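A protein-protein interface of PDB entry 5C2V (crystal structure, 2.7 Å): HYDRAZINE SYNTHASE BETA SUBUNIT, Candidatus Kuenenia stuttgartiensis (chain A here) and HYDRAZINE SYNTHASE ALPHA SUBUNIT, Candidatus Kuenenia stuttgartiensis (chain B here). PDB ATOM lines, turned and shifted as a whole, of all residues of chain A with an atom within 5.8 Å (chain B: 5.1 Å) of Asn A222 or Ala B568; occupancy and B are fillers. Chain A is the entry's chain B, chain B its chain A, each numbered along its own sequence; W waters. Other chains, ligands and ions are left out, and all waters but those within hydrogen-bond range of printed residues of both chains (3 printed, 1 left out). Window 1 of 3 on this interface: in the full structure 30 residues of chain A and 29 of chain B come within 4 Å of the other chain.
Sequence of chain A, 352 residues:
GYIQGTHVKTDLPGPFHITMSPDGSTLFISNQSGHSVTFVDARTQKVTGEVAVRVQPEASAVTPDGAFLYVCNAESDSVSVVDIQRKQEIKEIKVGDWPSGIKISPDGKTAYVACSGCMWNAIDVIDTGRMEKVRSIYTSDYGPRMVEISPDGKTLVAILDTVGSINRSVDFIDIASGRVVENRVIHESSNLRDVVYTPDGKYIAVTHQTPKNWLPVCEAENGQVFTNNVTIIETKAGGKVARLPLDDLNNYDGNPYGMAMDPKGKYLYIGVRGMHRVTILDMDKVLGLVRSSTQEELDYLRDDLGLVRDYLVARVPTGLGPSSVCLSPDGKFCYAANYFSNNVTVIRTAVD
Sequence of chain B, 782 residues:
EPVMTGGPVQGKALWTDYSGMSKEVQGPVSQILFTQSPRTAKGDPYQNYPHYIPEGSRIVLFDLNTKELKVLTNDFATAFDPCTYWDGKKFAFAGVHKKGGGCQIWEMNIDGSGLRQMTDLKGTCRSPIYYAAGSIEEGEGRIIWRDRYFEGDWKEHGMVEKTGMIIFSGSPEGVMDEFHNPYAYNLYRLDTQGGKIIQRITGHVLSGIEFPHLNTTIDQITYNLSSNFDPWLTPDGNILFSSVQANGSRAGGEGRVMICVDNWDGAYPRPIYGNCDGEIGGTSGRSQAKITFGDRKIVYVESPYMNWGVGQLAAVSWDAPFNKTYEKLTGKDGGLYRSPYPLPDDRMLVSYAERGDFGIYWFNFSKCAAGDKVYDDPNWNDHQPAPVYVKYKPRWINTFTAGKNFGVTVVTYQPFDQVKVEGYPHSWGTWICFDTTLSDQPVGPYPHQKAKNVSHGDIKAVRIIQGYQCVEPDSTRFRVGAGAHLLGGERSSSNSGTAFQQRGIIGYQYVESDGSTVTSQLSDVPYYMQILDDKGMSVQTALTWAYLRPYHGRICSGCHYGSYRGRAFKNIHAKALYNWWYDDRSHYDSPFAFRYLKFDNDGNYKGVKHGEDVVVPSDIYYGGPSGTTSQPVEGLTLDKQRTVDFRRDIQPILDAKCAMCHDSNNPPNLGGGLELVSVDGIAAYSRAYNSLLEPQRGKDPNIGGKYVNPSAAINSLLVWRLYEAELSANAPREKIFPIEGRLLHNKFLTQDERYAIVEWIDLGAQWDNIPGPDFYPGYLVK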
ATOM      1  N   LYS A 212      14.685 -26.972 -25.358  1.00  0.00           N
ATOM      2  CA  LYS A 212      15.481 -25.931 -24.743  1.00  0.00           C
ATOM      3  C   LYS A 212      16.115 -26.612 -23.541  1.00  0.00           C
ATOM      4  O   LYS A 212      15.468 -26.832 -22.517  1.00  0.00           O
ATOM      5  CB  LYS A 212      14.624 -24.729 -24.340  1.00  0.00           C
ATOM      6  CG  LYS A 212      13.333 -24.581 -25.149  1.00  0.00           C
ATOM      7  CD  LYS A 212      13.573 -24.103 -26.571  1.00  0.00           C
ATOM      8  CE  LYS A 212      12.262 -24.004 -27.341  1.00  0.00           C
ATOM      9  NZ  LYS A 212      12.436 -23.358 -28.672  1.00  0.00           N
ATOM     10  N   ALA A 220       4.889 -26.080 -18.967  1.00  0.00           N
ATOM     11  CA  ALA A 220       4.750 -26.717 -20.274  1.00  0.00           C
ATOM     12  C   ALA A 220       4.354 -25.744 -21.386  1.00  0.00           C
ATOM     13  O   ALA A 220       4.300 -26.122 -22.556  1.00  0.00           O
ATOM     14  CB  ALA A 220       3.741 -27.852 -20.193  1.00  0.00           C
ATOM     15  N   GLU A 221       4.082 -24.494 -21.025  1.00  0.00           N
ATOM     16  CA  GLU A 221       3.498 -23.547 -21.975  1.00  0.00           C
ATOM     17  C   GLU A 221       4.520 -22.924 -22.916  1.00  0.00           C
ATOM     18  O   GLU A 221       5.698 -22.796 -22.576  1.00  0.00           O
ATOM     19  CB  GLU A 221       2.738 -22.443 -21.235  1.00  0.00           C
ATOM     20  CG  GLU A 221       1.402 -22.887 -20.648  1.00  0.00           C
ATOM     21  CD  GLU A 221       1.535 -23.513 -19.272  1.00  0.00           C
ATOM     22  OE1 GLU A 221       2.657 -23.914 -18.903  1.00  0.00           O
ATOM     23  OE2 GLU A 221       0.513 -23.604 -18.558  1.00  0.00           O
ATOM     24  N   ASN A 222       4.047 -22.536 -24.098  1.00  0.00           N
ATOM     25  CA  ASN A 222       4.874 -21.886 -25.109  1.00  0.00           C
ATOM     26  C   ASN A 222       6.120 -22.694 -25.463  1.00  0.00           C
ATOM     27  O   ASN A 222       7.162 -22.124 -25.782  1.00  0.00           O
ATOM     28  CB  ASN A 222       5.278 -20.486 -24.645  1.00  0.00           C
ATOM     29  CG  ASN A 222       4.142 -19.485 -24.759  1.00  0.00           C
ATOM     30  OD1 ASN A 222       3.205 -19.496 -23.961  1.00  0.00           O
ATOM     31  ND2 ASN A 222       4.236 -18.595 -25.739  1.00  0.00           N
ATOM     32  N   GLY A 223       6.003 -24.018 -25.400  1.00  0.00           N
ATOM     33  CA  GLY A 223       7.100 -24.913 -25.722  1.00  0.00           C
ATOM     34  C   GLY A 223       8.380 -24.627 -24.960  1.00  0.00           C
ATOM     35  O   GLY A 223       9.458 -24.559 -25.551  1.00  0.00           O
ATOM     36  N   GLN A 224       8.262 -24.456 -23.646  1.00  0.00           N
ATOM     37  CA  GLN A 224       9.413 -24.120 -22.811  1.00  0.00           C
ATOM     38  C   GLN A 224      10.442 -25.245 -22.768  1.00  0.00           C
ATOM     39  O   GLN A 224      11.641 -25.000 -22.642  1.00  0.00           O
ATOM     40  CB  GLN A 224       8.969 -23.782 -21.385  1.00  0.00           C
ATOM     41  CG  GLN A 224      10.131 -23.425 -20.469  1.00  0.00           C
ATOM     42  CD  GLN A 224       9.878 -23.785 -19.023  1.00  0.00           C
ATOM     43  OE1 GLN A 224       8.739 -23.802 -18.566  1.00  0.00           O
ATOM     44  NE2 GLN A 224      10.945 -24.089 -18.297  1.00  0.00           N
ATOM     45  N   THR A 227       9.727 -28.060 -28.400  1.00  0.00           N
ATOM     46  CA  THR A 227       8.870 -27.676 -29.514  1.00  0.00           C
ATOM     47  C   THR A 227       9.072 -28.712 -30.606  1.00  0.00           C
ATOM     48  O   THR A 227      10.089 -29.396 -30.629  1.00  0.00           O
ATOM     49  CB  THR A 227       9.181 -26.268 -30.058  1.00  0.00           C
ATOM     50  OG1 THR A 227      10.496 -26.248 -30.627  1.00  0.00           O
ATOM     51  CG2 THR A 227       9.088 -25.230 -28.952  1.00  0.00           C
ATOM     52  N   LEU A 249      -0.049 -22.563 -30.539  1.00  0.00           N
ATOM     53  CA  LEU A 249       0.294 -22.088 -29.206  1.00  0.00           C
ATOM     54  C   LEU A 249      -0.132 -23.107 -28.158  1.00  0.00           C
ATOM     55  O   LEU A 249       0.673 -23.538 -27.335  1.00  0.00           O
ATOM     56  CB  LEU A 249      -0.361 -20.735 -28.919  1.00  0.00           C
ATOM     57  CG  LEU A 249      -0.085 -20.154 -27.530  1.00  0.00           C
ATOM     58  CD1 LEU A 249       1.385 -19.800 -27.372  1.00  0.00           C
ATOM     59  CD2 LEU A 249      -0.963 -18.944 -27.256  1.00  0.00           C
ATOM     60  N   TYR A 252       0.224 -28.866 -29.890  1.00  0.00           N
ATOM     61  CA  TYR A 252       1.548 -29.281 -30.343  1.00  0.00           C
ATOM     62  C   TYR A 252       1.482 -30.636 -31.038  1.00  0.00           C
ATOM     63  O   TYR A 252       0.604 -31.442 -30.738  1.00  0.00           O
ATOM     64  CB  TYR A 252       2.520 -29.344 -29.159  1.00  0.00           C
ATOM     65  CG  TYR A 252       2.776 -28.008 -28.495  1.00  0.00           C
ATOM     66  CD1 TYR A 252       1.802 -27.398 -27.717  1.00  0.00           C
ATOM     67  CD2 TYR A 252       3.996 -27.361 -28.636  1.00  0.00           C
ATOM     68  CE1 TYR A 252       2.029 -26.183 -27.112  1.00  0.00           C
ATOM     69  CE2 TYR A 252       4.232 -26.140 -28.033  1.00  0.00           C
ATOM     70  CZ  TYR A 252       3.244 -25.556 -27.273  1.00  0.00           C
ATOM     71  OH  TYR A 252       3.471 -24.343 -26.668  1.00  0.00           O
ATOM     72  N   ARG A 302      11.065 -19.493 -36.582  1.00  0.00           N
ATOM     73  CA  ARG A 302      11.036 -20.839 -36.012  1.00  0.00           C
ATOM     74  C   ARG A 302      10.202 -20.885 -34.734  1.00  0.00           C
ATOM     75  O   ARG A 302       9.507 -21.866 -34.470  1.00  0.00           O
ATOM     76  CB  ARG A 302      12.458 -21.333 -35.726  1.00  0.00           C
ATOM     77  CG  ARG A 302      12.529 -22.788 -35.277  1.00  0.00           C
ATOM     78  CD  ARG A 302      12.906 -22.907 -33.809  1.00  0.00           C
ATOM     79  NE  ARG A 302      14.349 -22.825 -33.603  1.00  0.00           N
ATOM     80  CZ  ARG A 302      14.930 -22.738 -32.410  1.00  0.00           C
ATOM     81  NH1 ARG A 302      14.190 -22.715 -31.311  1.00  0.00           N
ATOM     82  NH2 ARG A 302      16.250 -22.669 -32.316  1.00  0.00           N
ATOM     83  N   ASP A 303      10.269 -19.813 -33.952  1.00  0.00           N
ATOM     84  CA  ASP A 303       9.566 -19.742 -32.677  1.00  0.00           C
ATOM     85  C   ASP A 303       8.190 -19.092 -32.789  1.00  0.00           C
ATOM     86  O   ASP A 303       7.510 -18.898 -31.782  1.00  0.00           O
ATOM     87  CB  ASP A 303      10.408 -18.989 -31.647  1.00  0.00           C
ATOM     88  CG  ASP A 303      11.681 -19.726 -31.289  1.00  0.00           C
ATOM     89  OD1 ASP A 303      11.765 -20.938 -31.581  1.00  0.00           O
ATOM     90  OD2 ASP A 303      12.594 -19.098 -30.714  1.00  0.00           O
ATOM     91  N   ASP A 304       7.779 -18.754 -34.006  1.00  0.00           N
ATOM     92  CA  ASP A 304       6.453 -18.184 -34.201  1.00  0.00           C
ATOM     93  C   ASP A 304       5.442 -19.314 -34.058  1.00  0.00           C
ATOM     94  O   ASP A 304       5.481 -20.292 -34.804  1.00  0.00           O
ATOM     95  CB  ASP A 304       6.345 -17.517 -35.576  1.00  0.00           C
ATOM     96  CG  ASP A 304       5.073 -16.696 -35.740  1.00  0.00           C
ATOM     97  OD1 ASP A 304       4.107 -16.902 -34.976  1.00  0.00           O
ATOM     98  OD2 ASP A 304       5.041 -15.841 -36.649  1.00  0.00           O
ATOM     99  N   LEU A 305       4.532 -19.173 -33.100  1.00  0.00           N
ATOM    100  CA  LEU A 305       3.612 -20.255 -32.775  1.00  0.00           C
ATOM    101  C   LEU A 305       2.274 -20.097 -33.490  1.00  0.00           C
ATOM    102  O   LEU A 305       1.367 -20.912 -33.316  1.00  0.00           O
ATOM    103  CB  LEU A 305       3.411 -20.340 -31.259  1.00  0.00           C
ATOM    104  CG  LEU A 305       4.627 -20.906 -30.515  1.00  0.00           C
ATOM    105  CD1 LEU A 305       4.364 -21.041 -29.022  1.00  0.00           C
ATOM    106  CD2 LEU A 305       5.054 -22.244 -31.108  1.00  0.00           C
ATOM    107  N   ARG B 270      -1.178 -15.834 -18.012  1.00  0.00           N
ATOM    108  CA  ARG B 270      -0.637 -15.486 -19.322  1.00  0.00           C
ATOM    109  C   ARG B 270      -1.738 -14.959 -20.242  1.00  0.00           C
ATOM    110  O   ARG B 270      -2.887 -15.395 -20.156  1.00  0.00           O
ATOM    111  CB  ARG B 270       0.056 -16.696 -19.956  1.00  0.00           C
ATOM    112  CG  ARG B 270      -0.871 -17.859 -20.253  1.00  0.00           C
ATOM    113  CD  ARG B 270      -0.107 -19.092 -20.703  1.00  0.00           C
ATOM    114  NE  ARG B 270      -1.004 -20.209 -20.989  1.00  0.00           N
ATOM    115  CZ  ARG B 270      -1.432 -20.530 -22.206  1.00  0.00           C
ATOM    116  NH1 ARG B 270      -1.042 -19.823 -23.258  1.00  0.00           N
ATOM    117  NH2 ARG B 270      -2.250 -21.562 -22.372  1.00  0.00           N
ATOM    118  N   SER B 557      11.506 -15.317 -20.784  1.00  0.00           N
ATOM    119  CA  SER B 557      12.651 -15.232 -21.690  1.00  0.00           C
ATOM    120  C   SER B 557      13.187 -13.815 -21.803  1.00  0.00           C
ATOM    121  O   SER B 557      14.398 -13.599 -21.832  1.00  0.00           O
ATOM    122  CB  SER B 557      12.281 -15.730 -23.089  1.00  0.00           C
ATOM    123  OG  SER B 557      11.968 -17.108 -23.089  1.00  0.00           O
ATOM    124  N   TYR B 561       8.892 -10.237 -24.801  1.00  0.00           N
ATOM    125  CA  TYR B 561       9.478 -10.826 -26.008  1.00  0.00           C
ATOM    126  C   TYR B 561       8.538 -11.790 -26.738  1.00  0.00           C
ATOM    127  O   TYR B 561       8.748 -12.099 -27.912  1.00  0.00           O
ATOM    128  CB  TYR B 561      10.792 -11.543 -25.660  1.00  0.00           C
ATOM    129  CG  TYR B 561      11.292 -12.504 -26.723  1.00  0.00           C
ATOM    130  CD1 TYR B 561      11.935 -12.039 -27.864  1.00  0.00           C
ATOM    131  CD2 TYR B 561      11.122 -13.876 -26.582  1.00  0.00           C
ATOM    132  CE1 TYR B 561      12.394 -12.913 -28.834  1.00  0.00           C
ATOM    133  CE2 TYR B 561      11.576 -14.757 -27.547  1.00  0.00           C
ATOM    134  CZ  TYR B 561      12.212 -14.270 -28.671  1.00  0.00           C
ATOM    135  OH  TYR B 561      12.665 -15.144 -29.634  1.00  0.00           O
ATOM    136  N   GLY B 562       7.478 -12.233 -26.068  1.00  0.00           N
ATOM    137  CA  GLY B 562       6.589 -13.218 -26.661  1.00  0.00           C
ATOM    138  C   GLY B 562       6.630 -14.598 -26.025  1.00  0.00           C
ATOM    139  O   GLY B 562       5.847 -15.472 -26.398  1.00  0.00           O
ATOM    140  N   SER B 563       7.538 -14.806 -25.074  1.00  0.00           N
ATOM    141  CA  SER B 563       7.632 -16.099 -24.396  1.00  0.00           C
ATOM    142  C   SER B 563       6.362 -16.423 -23.619  1.00  0.00           C
ATOM    143  O   SER B 563       5.997 -17.589 -23.486  1.00  0.00           O
ATOM    144  CB  SER B 563       8.836 -16.140 -23.453  1.00  0.00           C
ATOM    145  OG  SER B 563       8.654 -15.278 -22.344  1.00  0.00           O
ATOM    146  N   TYR B 564       5.706 -15.404 -23.073  1.00  0.00           N
ATOM    147  CA  TYR B 564       4.399 -15.624 -22.464  1.00  0.00           C
ATOM    148  C   TYR B 564       3.225 -15.251 -23.375  1.00  0.00           C
ATOM    149  O   TYR B 564       2.074 -15.321 -22.943  1.00  0.00           O
ATOM    150  CB  TYR B 564       4.277 -14.889 -21.119  1.00  0.00           C
ATOM    151  CG  TYR B 564       4.853 -13.490 -21.034  1.00  0.00           C
ATOM    152  CD1 TYR B 564       4.081 -12.375 -21.344  1.00  0.00           C
ATOM    153  CD2 TYR B 564       6.151 -13.280 -20.585  1.00  0.00           C
ATOM    154  CE1 TYR B 564       4.600 -11.092 -21.243  1.00  0.00           C
ATOM    155  CE2 TYR B 564       6.679 -12.002 -20.481  1.00  0.00           C
ATOM    156  CZ  TYR B 564       5.899 -10.911 -20.809  1.00  0.00           C
ATOM    157  OH  TYR B 564       6.422  -9.637 -20.701  1.00  0.00           O
ATOM    158  N   ARG B 565       3.488 -14.851 -24.619  1.00  0.00           N
ATOM    159  CA  ARG B 565       2.370 -14.518 -25.502  1.00  0.00           C
ATOM    160  C   ARG B 565       2.241 -15.389 -26.760  1.00  0.00           C
ATOM    161  O   ARG B 565       1.463 -16.343 -26.774  1.00  0.00           O
ATOM    162  CB  ARG B 565       2.481 -13.044 -25.916  1.00  0.00           C
ATOM    163  CG  ARG B 565       1.429 -12.555 -26.910  1.00  0.00           C
ATOM    164  CD  ARG B 565       0.020 -12.664 -26.360  1.00  0.00           C
ATOM    165  NE  ARG B 565      -0.977 -12.301 -27.363  1.00  0.00           N
ATOM    166  CZ  ARG B 565      -1.533 -13.162 -28.208  1.00  0.00           C
ATOM    167  NH1 ARG B 565      -1.192 -14.443 -28.171  1.00  0.00           N
ATOM    168  NH2 ARG B 565      -2.433 -12.746 -29.088  1.00  0.00           N
ATOM    169  N   GLY B 566       2.999 -15.071 -27.808  1.00  0.00           N
ATOM    170  CA  GLY B 566       2.877 -15.788 -29.066  1.00  0.00           C
ATOM    171  C   GLY B 566       4.078 -16.585 -29.535  1.00  0.00           C
ATOM    172  O   GLY B 566       4.053 -17.165 -30.622  1.00  0.00           O
ATOM    173  N   ARG B 567       5.124 -16.633 -28.722  1.00  0.00           N
ATOM    174  CA  ARG B 567       6.385 -17.202 -29.177  1.00  0.00           C
ATOM    175  C   ARG B 567       6.911 -18.263 -28.225  1.00  0.00           C
ATOM    176  O   ARG B 567       6.600 -18.259 -27.035  1.00  0.00           O
ATOM    177  CB  ARG B 567       7.434 -16.099 -29.360  1.00  0.00           C
ATOM    178  CG  ARG B 567       7.205 -15.218 -30.578  1.00  0.00           C
ATOM    179  CD  ARG B 567       8.288 -14.157 -30.722  1.00  0.00           C
ATOM    180  NE  ARG B 567       9.625 -14.731 -30.846  1.00  0.00           N
ATOM    181  CZ  ARG B 567      10.124 -15.236 -31.971  1.00  0.00           C
ATOM    182  NH1 ARG B 567       9.396 -15.246 -33.079  1.00  0.00           N
ATOM    183  NH2 ARG B 567      11.353 -15.735 -31.988  1.00  0.00           N
ATOM    184  N   ALA B 568       7.709 -19.176 -28.763  1.00  0.00           N
ATOM    185  CA  ALA B 568       8.332 -20.208 -27.955  1.00  0.00           C
ATOM    186  C   ALA B 568       9.450 -19.612 -27.111  1.00  0.00           C
ATOM    187  O   ALA B 568      10.045 -18.600 -27.484  1.00  0.00           O
ATOM    188  CB  ALA B 568       8.865 -21.329 -28.834  1.00  0.00           C
ATOM    189  N   PHE B 569       9.721 -20.235 -25.970  1.00  0.00           N
ATOM    190  CA  PHE B 569      10.827 -19.819 -25.121  1.00  0.00           C
ATOM    191  C   PHE B 569      12.139 -19.893 -25.892  1.00  0.00           C
ATOM    192  O   PHE B 569      12.392 -20.857 -26.614  1.00  0.00           O
ATOM    193  CB  PHE B 569      10.903 -20.686 -23.863  1.00  0.00           C
ATOM    194  CG  PHE B 569      10.024 -20.212 -22.741  1.00  0.00           C
ATOM    195  CD1 PHE B 569      10.543 -19.429 -21.724  1.00  0.00           C
ATOM    196  CD2 PHE B 569       8.682 -20.556 -22.696  1.00  0.00           C
ATOM    197  CE1 PHE B 569       9.743 -18.991 -20.686  1.00  0.00           C
ATOM    198  CE2 PHE B 569       7.876 -20.123 -21.657  1.00  0.00           C
ATOM    199  CZ  PHE B 569       8.408 -19.339 -20.651  1.00  0.00           C
ATOM    200  N   LYS B 570      12.963 -18.863 -25.747  1.00  0.00           N
ATOM    201  CA  LYS B 570      14.263 -18.836 -26.402  1.00  0.00           C
ATOM    202  C   LYS B 570      15.268 -19.618 -25.573  1.00  0.00           C
ATOM    203  O   LYS B 570      15.280 -19.513 -24.346  1.00  0.00           O
ATOM    204  CB  LYS B 570      14.735 -17.394 -26.600  1.00  0.00           C
ATOM    205  CG  LYS B 570      16.046 -17.262 -27.354  1.00  0.00           C
ATOM    206  CD  LYS B 570      16.413 -15.801 -27.557  1.00  0.00           C
ATOM    207  CE  LYS B 570      17.670 -15.659 -28.397  1.00  0.00           C
ATOM    208  NZ  LYS B 570      18.035 -14.231 -28.603  1.00  0.00           N
HETATM  209  O   HOH W   1       4.199 -18.991 -21.679  1.00  0.00           O
HETATM  210  O   HOH W   2      -1.376 -21.885 -19.007  1.00  0.00           O
HETATM  211  O   HOH W   3       1.066 -18.175 -23.618  1.00  0.00           O
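The backbone carbonyl oxygen (O) of Ser B563 sits close to the side-chain amide nitrogen (ND2) of Asn A222 (3.0 Å). O of Gly B566 is in hydrogen-bond range of N of Leu A305. The side-chain amide nitrogen of Asn A222 is in hydrogen-bond range of the backbone carbonyl oxygen of Arg B567 (2.7 Å). NH2 of Arg B567 is in salt-bridge range of OD2 of Asp A303 (3.8 Å). N of Ala B568 is in hydrogen-bond range of O of Asp A303 (3.0 Å). The backbone carbonyl oxygen (O) of Phe B569 lies close to the side-chain amino group (NZ) of Lys A212 (3.2 Å). The backbone NH (N) of Phe B569 lies within hydrogen-bond range of the backbone carbonyl oxygen (O) of Asn A222 (3.2 Å).
N of Ser B557 sits at hydrogen-bond distance from OG of Ser B563 (3.3 Å). The guanidinium group (NH2) of Arg B567 is in hydrogen-bond range of the side-chain hydroxyl (OH) of Tyr B561 (2.8 Å). NZ of Lys A212 lies within salt-bridge range of OD1 of Asp A303. The side-chain hydroxyl of Tyr A252 is in hydrogen-bond range of the backbone NH of Asn A222, at 3.2 Å. The backbone carbonyl oxygen (O) of Leu A249 lies close to the side-chain hydroxyl (OH) of Tyr A252 (3.0 Å). The guanidinium group (NH1) of Arg A302 lies within salt-bridge range of the side-chain carboxylate (OD1) of Asp A303 (3.0 Å).
Arg B270 touches Glu A221 (NE to CG, 3.6 Å). Phe B569 touches Glu A221 (CE2 to O, 3.6 Å). ND2 of Asn A222 touches O of Gly B562, at 3.6 Å. O of Arg B565 touches ND2 of Asn A222, at 3.7 Å. CA of Ala B568 touches O of Asn A222 (3.1 Å). Phe B569 touches Gln A224 (CD2 to CB, 3.5 Å). Leu A249 touches Arg B565. Arg B567 touches Asp A304. C of Arg B567 touches CD1 of Leu A305 (3.9 Å). N of Ala B568 touches CD1 of Leu A305 (3.8 Å).
Of chain A, only Asn A222 (3.1 Å), Thr A227 (3.9 Å), Asp A303 (3.0 Å) and Leu A305 (3.8 Å) come within 4 Å of Ala B568. Of the printed residues of chain A, Phe B569 touches Lys A212, Glu A221, Asn A222 and Gln A224. Of the printed residues of chain B, Thr A227 touches Ala B568. The nearest residue of chain A that does not touch Ala B568 is Lys A212 (4.1 Å). The nearest printed residue of chain B that does not touch Lys A212 is Ala B568 (4.1 Å).
Hydrophobic or aromatic side chains of chain B that line the printed part of chain A: Ala B568 and Phe B569. Printed residues of chain A that touch a printed residue of chain B: Lys A212, Glu A221, Asn A222, Gln A224, Thr A227, Leu A249, Asp A303, Asp A304 and Leu A305. Along chain A the printed residues that touch a printed residue of chain B span positions 212 to 305. Among the printed residues, 18 pairs touch across the chains.
Water W3 lies within hydrogen-bond range of the side-chain amide oxygen (OD1) of Asn A222 (2.5 Å), the guanidinium group (NH1) of Arg B270 (2.7 Å) and the backbone carbonyl oxygen (O) of Tyr B564 (3.1 Å). Water W1 lies within hydrogen-bond range of the side-chain amide oxygen (OD1) of Asn A222 and the backbone carbonyl oxygen (O) of Ser B563. Water W2 bridges OE2 of Glu A221 (2.6 Å) and NE of Arg B270 (2.6 Å).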
